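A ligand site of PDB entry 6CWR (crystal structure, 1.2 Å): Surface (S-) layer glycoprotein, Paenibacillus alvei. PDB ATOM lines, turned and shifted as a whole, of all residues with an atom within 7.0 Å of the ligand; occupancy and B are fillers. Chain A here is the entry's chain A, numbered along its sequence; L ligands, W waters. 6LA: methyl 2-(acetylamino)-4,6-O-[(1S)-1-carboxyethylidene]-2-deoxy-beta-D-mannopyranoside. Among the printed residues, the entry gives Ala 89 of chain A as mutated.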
ATOM      1  N   ARG A  41      19.885  -8.491 -18.342  1.00  0.00           N
ATOM      2  CA  ARG A  41      21.020  -8.055 -19.156  1.00  0.00           C
ATOM      3  C   ARG A  41      22.378  -8.238 -18.449  1.00  0.00           C
ATOM      4  O   ARG A  41      23.368  -8.618 -19.071  1.00  0.00           O
ATOM      5  CB  ARG A  41      20.782  -6.625 -19.633  1.00  0.00           C
ATOM      6  CG  ARG A  41      19.676  -6.523 -20.679  1.00  0.00           C
ATOM      7  CD  ARG A  41      19.152  -5.115 -20.950  1.00  0.00           C
ATOM      8  NE  ARG A  41      20.188  -4.156 -21.292  1.00  0.00           N
ATOM      9  CZ  ARG A  41      20.845  -4.098 -22.460  1.00  0.00           C
ATOM     10  NH1 ARG A  41      20.527  -4.915 -23.463  1.00  0.00           N
ATOM     11  NH2 ARG A  41      21.810  -3.186 -22.640  1.00  0.00           N
ATOM     12  N   TYR A  63      28.562   3.423 -17.299  1.00  0.00           N
ATOM     13  CA  TYR A  63      27.133   3.679 -17.259  1.00  0.00           C
ATOM     14  C   TYR A  63      26.788   4.397 -15.950  1.00  0.00           C
ATOM     15  O   TYR A  63      27.507   4.328 -14.949  1.00  0.00           O
ATOM     16  CB  TYR A  63      26.367   2.356 -17.363  1.00  0.00           C
ATOM     17  CG  TYR A  63      26.701   1.651 -18.634  1.00  0.00           C
ATOM     18  CD1 TYR A  63      26.239   2.119 -19.832  1.00  0.00           C
ATOM     19  CD2 TYR A  63      27.561   0.560 -18.649  1.00  0.00           C
ATOM     20  CE1 TYR A  63      26.555   1.490 -21.022  1.00  0.00           C
ATOM     21  CE2 TYR A  63      27.885  -0.073 -19.816  1.00  0.00           C
ATOM     22  CZ  TYR A  63      27.403   0.406 -21.022  1.00  0.00           C
ATOM     23  OH  TYR A  63      27.747  -0.208 -22.212  1.00  0.00           O
ATOM     24  N   GLY A  85      32.437  -4.427 -27.768  1.00  0.00           N
ATOM     25  CA  GLY A  85      31.492  -3.956 -28.770  1.00  0.00           C
ATOM     26  C   GLY A  85      30.243  -4.816 -28.908  1.00  0.00           C
ATOM     27  O   GLY A  85      29.500  -4.671 -29.858  1.00  0.00           O
ATOM     28  N   LEU A  86      29.978  -5.709 -27.953  1.00  0.00           N
ATOM     29  CA  LEU A  86      28.819  -6.576 -28.035  1.00  0.00           C
ATOM     30  C   LEU A  86      27.537  -5.942 -27.466  1.00  0.00           C
ATOM     31  O   LEU A  86      26.449  -6.235 -27.977  1.00  0.00           O
ATOM     32  CB  LEU A  86      29.060  -7.886 -27.295  1.00  0.00           C
ATOM     33  CG  LEU A  86      30.265  -8.693 -27.747  1.00  0.00           C
ATOM     34  CD1 LEU A  86      30.365 -10.031 -27.028  1.00  0.00           C
ATOM     35  CD2 LEU A  86      30.386  -8.863 -29.243  1.00  0.00           C
ATOM     36  N   MET A  87      27.666  -5.154 -26.411  1.00  0.00           N
ATOM     37  CA  MET A  87      26.545  -4.491 -25.766  1.00  0.00           C
ATOM     38  C   MET A  87      26.933  -3.029 -25.542  1.00  0.00           C
ATOM     39  O   MET A  87      28.098  -2.670 -25.415  1.00  0.00           O
ATOM     40  CB  MET A  87      26.131  -5.150 -24.464  1.00  0.00           C
ATOM     41  CG  MET A  87      25.705  -6.591 -24.659  1.00  0.00           C
ATOM     42  SD  MET A  87      25.103  -7.421 -23.147  1.00  0.00           S
ATOM     43  CE  MET A  87      23.410  -6.810 -23.044  1.00  0.00           C
ATOM     44  N   GLN A  88      25.924  -2.200 -25.457  1.00  0.00           N
ATOM     45  CA  GLN A  88      26.100  -0.781 -25.204  1.00  0.00           C
ATOM     46  C   GLN A  88      24.860  -0.266 -24.486  1.00  0.00           C
ATOM     47  O   GLN A  88      23.952  -1.015 -24.149  1.00  0.00           O
ATOM     48  CB  GLN A  88      26.336  -0.019 -26.517  1.00  0.00           C
ATOM     49  CG  GLN A  88      25.104   0.014 -27.416  1.00  0.00           C
ATOM     50  CD  GLN A  88      25.258   0.715 -28.771  1.00  0.00           C
ATOM     51  OE1 GLN A  88      24.446   0.476 -29.689  1.00  0.00           O
ATOM     52  NE2 GLN A  88      26.259   1.580 -28.913  1.00  0.00           N
ATOM     53  N   ALA A  89      24.810   1.040 -24.272  1.00  0.00           N
ATOM     54  CA  ALA A  89      23.688   1.616 -23.581  1.00  0.00           C
ATOM     55  C   ALA A  89      22.406   1.472 -24.396  1.00  0.00           C
ATOM     56  O   ALA A  89      22.443   1.371 -25.640  1.00  0.00           O
ATOM     57  CB  ALA A  89      23.950   3.092 -23.323  1.00  0.00           C
ATOM     58  N   LYS A  90      21.265   1.506 -23.702  1.00  0.00           N
ATOM     59  CA  LYS A  90      20.003   1.796 -24.355  1.00  0.00           C
ATOM     60  C   LYS A  90      19.802   3.305 -24.617  1.00  0.00           C
ATOM     61  O   LYS A  90      19.043   3.678 -25.524  1.00  0.00           O
ATOM     62  CB  LYS A  90      18.854   1.291 -23.500  1.00  0.00           C
ATOM     63  CG  LYS A  90      18.770  -0.206 -23.346  1.00  0.00           C
ATOM     64  CD  LYS A  90      17.438  -0.613 -22.747  1.00  0.00           C
ATOM     65  CE  LYS A  90      17.331  -2.127 -22.681  1.00  0.00           C
ATOM     66  NZ  LYS A  90      16.083  -2.574 -22.012  1.00  0.00           N
ATOM     67  N   ASP A  91      20.494   4.145 -23.850  1.00  0.00           N
ATOM     68  CA  ASP A  91      20.345   5.594 -23.935  1.00  0.00           C
ATOM     69  C   ASP A  91      21.736   6.163 -23.833  1.00  0.00           C
ATOM     70  O   ASP A  91      22.343   6.123 -22.756  1.00  0.00           O
ATOM     71  CB  ASP A  91      19.472   6.070 -22.750  1.00  0.00           C
ATOM     72  CG  ASP A  91      19.230   7.569 -22.713  1.00  0.00           C
ATOM     73  OD1 ASP A  91      20.012   8.353 -23.296  1.00  0.00           O
ATOM     74  OD2 ASP A  91      18.243   7.935 -22.027  1.00  0.00           O
ATOM     75  N   LEU A  92      22.236   6.698 -24.953  1.00  0.00           N
ATOM     76  CA  LEU A  92      23.583   7.270 -25.034  1.00  0.00           C
ATOM     77  C   LEU A  92      23.731   8.673 -24.428  1.00  0.00           C
ATOM     78  O   LEU A  92      24.857   9.181 -24.288  1.00  0.00           O
ATOM     79  CB  LEU A  92      24.016   7.363 -26.508  1.00  0.00           C
ATOM     80  CG  LEU A  92      24.057   6.066 -27.302  1.00  0.00           C
ATOM     81  CD1 LEU A  92      24.176   6.312 -28.805  1.00  0.00           C
ATOM     82  CD2 LEU A  92      25.227   5.267 -26.811  1.00  0.00           C
ATOM     83  N   PHE A  97      22.497   1.467 -19.162  1.00  0.00           N
ATOM     84  CA  PHE A  97      22.599   0.139 -19.718  1.00  0.00           C
ATOM     85  C   PHE A  97      21.324  -0.689 -19.501  1.00  0.00           C
ATOM     86  O   PHE A  97      21.062  -1.624 -20.251  1.00  0.00           O
ATOM     87  CB  PHE A  97      23.793  -0.573 -19.027  1.00  0.00           C
ATOM     88  CG  PHE A  97      24.127  -1.940 -19.607  1.00  0.00           C
ATOM     89  CD1 PHE A  97      24.814  -2.009 -20.807  1.00  0.00           C
ATOM     90  CD2 PHE A  97      23.754  -3.128 -18.979  1.00  0.00           C
ATOM     91  CE1 PHE A  97      25.180  -3.192 -21.354  1.00  0.00           C
ATOM     92  CE2 PHE A  97      24.163  -4.355 -19.552  1.00  0.00           C
ATOM     93  CZ  PHE A  97      24.821  -4.358 -20.741  1.00  0.00           C
ATOM     94  N   ILE A 103      16.931  -9.359 -20.910  1.00  0.00           N
ATOM     95  CA  ILE A 103      17.450  -9.389 -22.282  1.00  0.00           C
ATOM     96  C   ILE A 103      16.369  -9.893 -23.230  1.00  0.00           C
ATOM     97  O   ILE A 103      15.705 -10.904 -22.951  1.00  0.00           O
ATOM     98  CB  ILE A 103      18.724 -10.239 -22.337  1.00  0.00           C
ATOM     99  CG1 ILE A 103      19.453 -10.151 -23.670  1.00  0.00           C
ATOM    100  CG2 ILE A 103      18.468 -11.730 -22.069  1.00  0.00           C
ATOM    101  CD1 ILE A 103      20.400  -9.049 -23.802  1.00  0.00           C
ATOM    102  N   THR A 104      16.185  -9.196 -24.345  1.00  0.00           N
ATOM    103  CA  THR A 104      15.210  -9.641 -25.314  1.00  0.00           C
ATOM    104  C   THR A 104      15.864 -10.492 -26.392  1.00  0.00           C
ATOM    105  O   THR A 104      17.067 -10.535 -26.551  1.00  0.00           O
ATOM    106  CB  THR A 104      14.481  -8.458 -25.941  1.00  0.00           C
ATOM    107  OG1 THR A 104      15.410  -7.677 -26.686  1.00  0.00           O
ATOM    108  CG2 THR A 104      13.792  -7.637 -24.845  1.00  0.00           C
ATOM    109  N   GLU A 106      15.797 -10.036 -29.646  1.00  0.00           N
ATOM    110  CA  GLU A 106      16.537  -9.236 -30.607  1.00  0.00           C
ATOM    111  C   GLU A 106      17.829  -8.661 -30.028  1.00  0.00           C
ATOM    112  O   GLU A 106      18.797  -8.521 -30.754  1.00  0.00           O
ATOM    113  CB  GLU A 106      15.646  -8.139 -31.213  1.00  0.00           C
ATOM    114  CG  GLU A 106      15.186  -7.031 -30.250  1.00  0.00           C
ATOM    115  CD  GLU A 106      14.091  -6.133 -30.765  1.00  0.00           C
ATOM    116  OE1 GLU A 106      13.560  -6.413 -31.846  1.00  0.00           O
ATOM    117  OE2 GLU A 106      13.720  -5.172 -30.050  1.00  0.00           O
ATOM    118  N   GLU A 107      17.853  -8.305 -28.767  1.00  0.00           N
ATOM    119  CA  GLU A 107      19.091  -7.844 -28.113  1.00  0.00           C
ATOM    120  C   GLU A 107      20.135  -8.963 -28.112  1.00  0.00           C
ATOM    121  O   GLU A 107      21.305  -8.764 -28.491  1.00  0.00           O
ATOM    122  CB  GLU A 107      18.794  -7.332 -26.712  1.00  0.00           C
ATOM    123  CG  GLU A 107      18.070  -6.011 -26.652  1.00  0.00           C
ATOM    124  CD  GLU A 107      17.647  -5.646 -25.239  1.00  0.00           C
ATOM    125  OE1 GLU A 107      17.875  -6.462 -24.298  1.00  0.00           O
ATOM    126  OE2 GLU A 107      17.124  -4.522 -25.060  1.00  0.00           O
ATOM    127  N   ALA A 108      19.715 -10.142 -27.673  1.00  0.00           N
ATOM    128  CA  ALA A 108      20.633 -11.277 -27.689  1.00  0.00           C
ATOM    129  C   ALA A 108      21.137 -11.560 -29.100  1.00  0.00           C
ATOM    130  O   ALA A 108      22.325 -11.873 -29.301  1.00  0.00           O
ATOM    131  CB  ALA A 108      19.984 -12.501 -27.083  1.00  0.00           C
ATOM    132  N   SER A 109      20.229 -11.426 -30.071  1.00  0.00           N
ATOM    133  CA  SER A 109      20.613 -11.606 -31.477  1.00  0.00           C
ATOM    134  C   SER A 109      21.734 -10.656 -31.858  1.00  0.00           C
ATOM    135  O   SER A 109      22.709 -11.101 -32.484  1.00  0.00           O
ATOM    136  CB  SER A 109      19.406 -11.368 -32.412  1.00  0.00           C
ATOM    137  OG  SER A 109      18.403 -12.354 -32.262  1.00  0.00           O
ATOM    138  N   LYS A 110      21.606  -9.358 -31.548  1.00  0.00           N
ATOM    139  CA  LYS A 110      22.673  -8.413 -31.874  1.00  0.00           C
ATOM    140  C   LYS A 110      24.005  -8.878 -31.265  1.00  0.00           C
ATOM    141  O   LYS A 110      25.032  -8.843 -31.932  1.00  0.00           O
ATOM    142  CB  LYS A 110      22.336  -6.995 -31.363  1.00  0.00           C
ATOM    143  CG  LYS A 110      23.500  -6.024 -31.535  1.00  0.00           C
ATOM    144  CD  LYS A 110      23.216  -4.622 -30.990  1.00  0.00           C
ATOM    145  CE  LYS A 110      24.507  -3.820 -30.844  1.00  0.00           C
ATOM    146  NZ  LYS A 110      24.518  -2.950 -29.664  1.00  0.00           N
ATOM    147  N   THR A 111      23.993  -9.249 -29.994  1.00  0.00           N
ATOM    148  CA  THR A 111      25.271  -9.601 -29.324  1.00  0.00           C
ATOM    149  C   THR A 111      25.951 -10.772 -30.024  1.00  0.00           C
ATOM    150  O   THR A 111      27.167 -10.769 -30.170  1.00  0.00           O
ATOM    151  CB  THR A 111      25.081  -9.897 -27.807  1.00  0.00           C
ATOM    152  OG1 THR A 111      24.425 -11.166 -27.587  1.00  0.00           O
ATOM    153  CG2 THR A 111      24.338  -8.756 -27.124  1.00  0.00           C
ATOM    154  N   THR A 129      12.100  -4.675 -33.605  1.00  0.00           N
ATOM    155  CA  THR A 129      12.252  -3.224 -33.509  1.00  0.00           C
ATOM    156  C   THR A 129      13.165  -2.748 -34.643  1.00  0.00           C
ATOM    157  O   THR A 129      14.111  -3.470 -35.021  1.00  0.00           O
ATOM    158  CB  THR A 129      12.831  -2.846 -32.133  1.00  0.00           C
ATOM    159  OG1 THR A 129      12.058  -3.488 -31.118  1.00  0.00           O
ATOM    160  CG2 THR A 129      12.762  -1.330 -31.910  1.00  0.00           C
ATOM    161  N   TRP A 131      15.806  -0.861 -35.214  1.00  0.00           N
ATOM    162  CA  TRP A 131      17.270  -0.974 -35.061  1.00  0.00           C
ATOM    163  C   TRP A 131      17.792  -2.400 -35.133  1.00  0.00           C
ATOM    164  O   TRP A 131      18.945  -2.614 -35.493  1.00  0.00           O
ATOM    165  CB  TRP A 131      17.742  -0.296 -33.736  1.00  0.00           C
ATOM    166  CG  TRP A 131      17.336  -1.015 -32.476  1.00  0.00           C
ATOM    167  CD1 TRP A 131      16.291  -0.707 -31.680  1.00  0.00           C
ATOM    168  CD2 TRP A 131      17.963  -2.184 -31.891  1.00  0.00           C
ATOM    169  NE1 TRP A 131      16.207  -1.583 -30.641  1.00  0.00           N
ATOM    170  CE2 TRP A 131      17.219  -2.507 -30.754  1.00  0.00           C
ATOM    171  CE3 TRP A 131      19.082  -2.981 -32.223  1.00  0.00           C
ATOM    172  CZ2 TRP A 131      17.539  -3.608 -29.946  1.00  0.00           C
ATOM    173  CZ3 TRP A 131      19.385  -4.077 -31.416  1.00  0.00           C
ATOM    174  CH2 TRP A 131      18.609  -4.370 -30.291  1.00  0.00           C
ATOM    175  N   TYR A 135      19.879  -7.535 -37.375  1.00  0.00           N
ATOM    176  CA  TYR A 135      20.514  -8.464 -36.426  1.00  0.00           C
ATOM    177  C   TYR A 135      19.649  -9.690 -36.222  1.00  0.00           C
ATOM    178  O   TYR A 135      20.159 -10.827 -36.214  1.00  0.00           O
ATOM    179  CB  TYR A 135      20.785  -7.767 -35.083  1.00  0.00           C
ATOM    180  CG  TYR A 135      21.852  -6.705 -35.132  1.00  0.00           C
ATOM    181  CD1 TYR A 135      23.173  -7.022 -35.409  1.00  0.00           C
ATOM    182  CD2 TYR A 135      21.564  -5.386 -34.776  1.00  0.00           C
ATOM    183  CE1 TYR A 135      24.161  -6.052 -35.440  1.00  0.00           C
ATOM    184  CE2 TYR A 135      22.554  -4.420 -34.764  1.00  0.00           C
ATOM    185  CZ  TYR A 135      23.842  -4.763 -35.118  1.00  0.00           C
ATOM    186  OH  TYR A 135      24.843  -3.842 -35.114  1.00  0.00           O
HETATM  187  C8  6LA L   1      22.450   3.146 -28.378  1.00  0.00           C
HETATM  188  C7  6LA L   1      21.615   2.158 -29.157  1.00  0.00           C
HETATM  189  O7  6LA L   1      21.387   2.385 -30.352  1.00  0.00           O
HETATM  190  N2  6LA L   1      21.184   1.070 -28.464  1.00  0.00           N
HETATM  191  C2  6LA L   1      20.278   0.103 -29.117  1.00  0.00           C
HETATM  192  C3  6LA L   1      20.919  -1.276 -29.343  1.00  0.00           C
HETATM  193  O3  6LA L   1      22.113  -1.118 -30.088  1.00  0.00           O
HETATM  194  C4  6LA L   1      21.151  -1.989 -28.062  1.00  0.00           C
HETATM  195  O4  6LA L   1      21.542  -3.364 -28.326  1.00  0.00           O
HETATM  196  CAB 6LA L   1      21.725  -4.105 -27.147  1.00  0.00           C
HETATM  197  CAK 6LA L   1      21.996  -5.556 -27.580  1.00  0.00           C
HETATM  198  CAL 6LA L   1      22.941  -3.639 -26.363  1.00  0.00           C
HETATM  199  OAN 6LA L   1      23.852  -3.118 -27.010  1.00  0.00           O
HETATM  200  OAM 6LA L   1      22.931  -3.910 -25.172  1.00  0.00           O
HETATM  201  O6  6LA L   1      20.573  -4.067 -26.314  1.00  0.00           O
HETATM  202  C6  6LA L   1      20.140  -2.782 -25.952  1.00  0.00           C
HETATM  203  C5  6LA L   1      19.900  -2.044 -27.265  1.00  0.00           C
HETATM  204  O5  6LA L   1      19.440  -0.716 -27.001  1.00  0.00           O
HETATM  205  C1  6LA L   1      19.016  -0.105 -28.248  1.00  0.00           C
HETATM  206  O1  6LA L   1      18.457   1.134 -27.872  1.00  0.00           O
HETATM  207  CAU 6LA L   1      17.160   1.035 -27.262  1.00  0.00           C
HETATM  208  O   HOH W   1      21.899  -0.395 -32.766  1.00  0.00           O
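The backbone carbonyl oxygen of Ala 89 sits at hydrogen-bond distance from a nitrogen (N2) of the ligand (3.1 Å).
The side-chain amino group (NZ) of Lys 110 lies within salt-bridge range of an oxygen (OAN) of the ligand, at 2.7 Å.
NH2 of Arg 41 lies within salt-bridge range of OAM of the ligand (2.9 Å).
The backbone NH (N) of Gln 88 is in hydrogen-bond range of an oxygen (OAN) of the ligand (2.7 Å).
An oxygen (O3) of the ligand sits at hydrogen-bond distance from the side-chain amide oxygen of Gln 88, 2.9 Å away.
The side-chain amide oxygen (OE1) of Gln 88 lies within hydrogen-bond range of the side-chain amino group (NZ) of Lys 110 (3.4 Å).
NH2 of Arg 41 is in hydrogen-bond range of O of Gln 88 (3.4 Å).
NE of Arg 41 lies within hydrogen-bond range of O of Phe 97 (2.9 Å).
The guanidinium group of Arg 41 lies within salt-bridge range of the side-chain carboxylate of Glu 107, at 3.2 Å.
OE1 of Glu 107 lies within hydrogen-bond range of N of Thr 104.
NZ of Lys 90 is in salt-bridge range of OE2 of Glu 107 (3.8 Å).
OG1 of Thr 111 sits at hydrogen-bond distance from O of Ala 108 (2.8 Å).
Met 87 touches the ligand (CA to OAN, 3.3 Å).
O of Lys 90 touches O1 of the ligand (3.5 Å).
Leu 92 touches the ligand.
CG of Glu 107 touches O6 of the ligand, 3.2 Å away.
Thr 111 touches the ligand (CG2 to CAK, 3.99 Å).
CH2 of Trp 131 touches O4 of the ligand (3.7 Å).
Hydrophobic or aromatic side chains that line the ligand: Met 87, Leu 92 and Trp 131.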
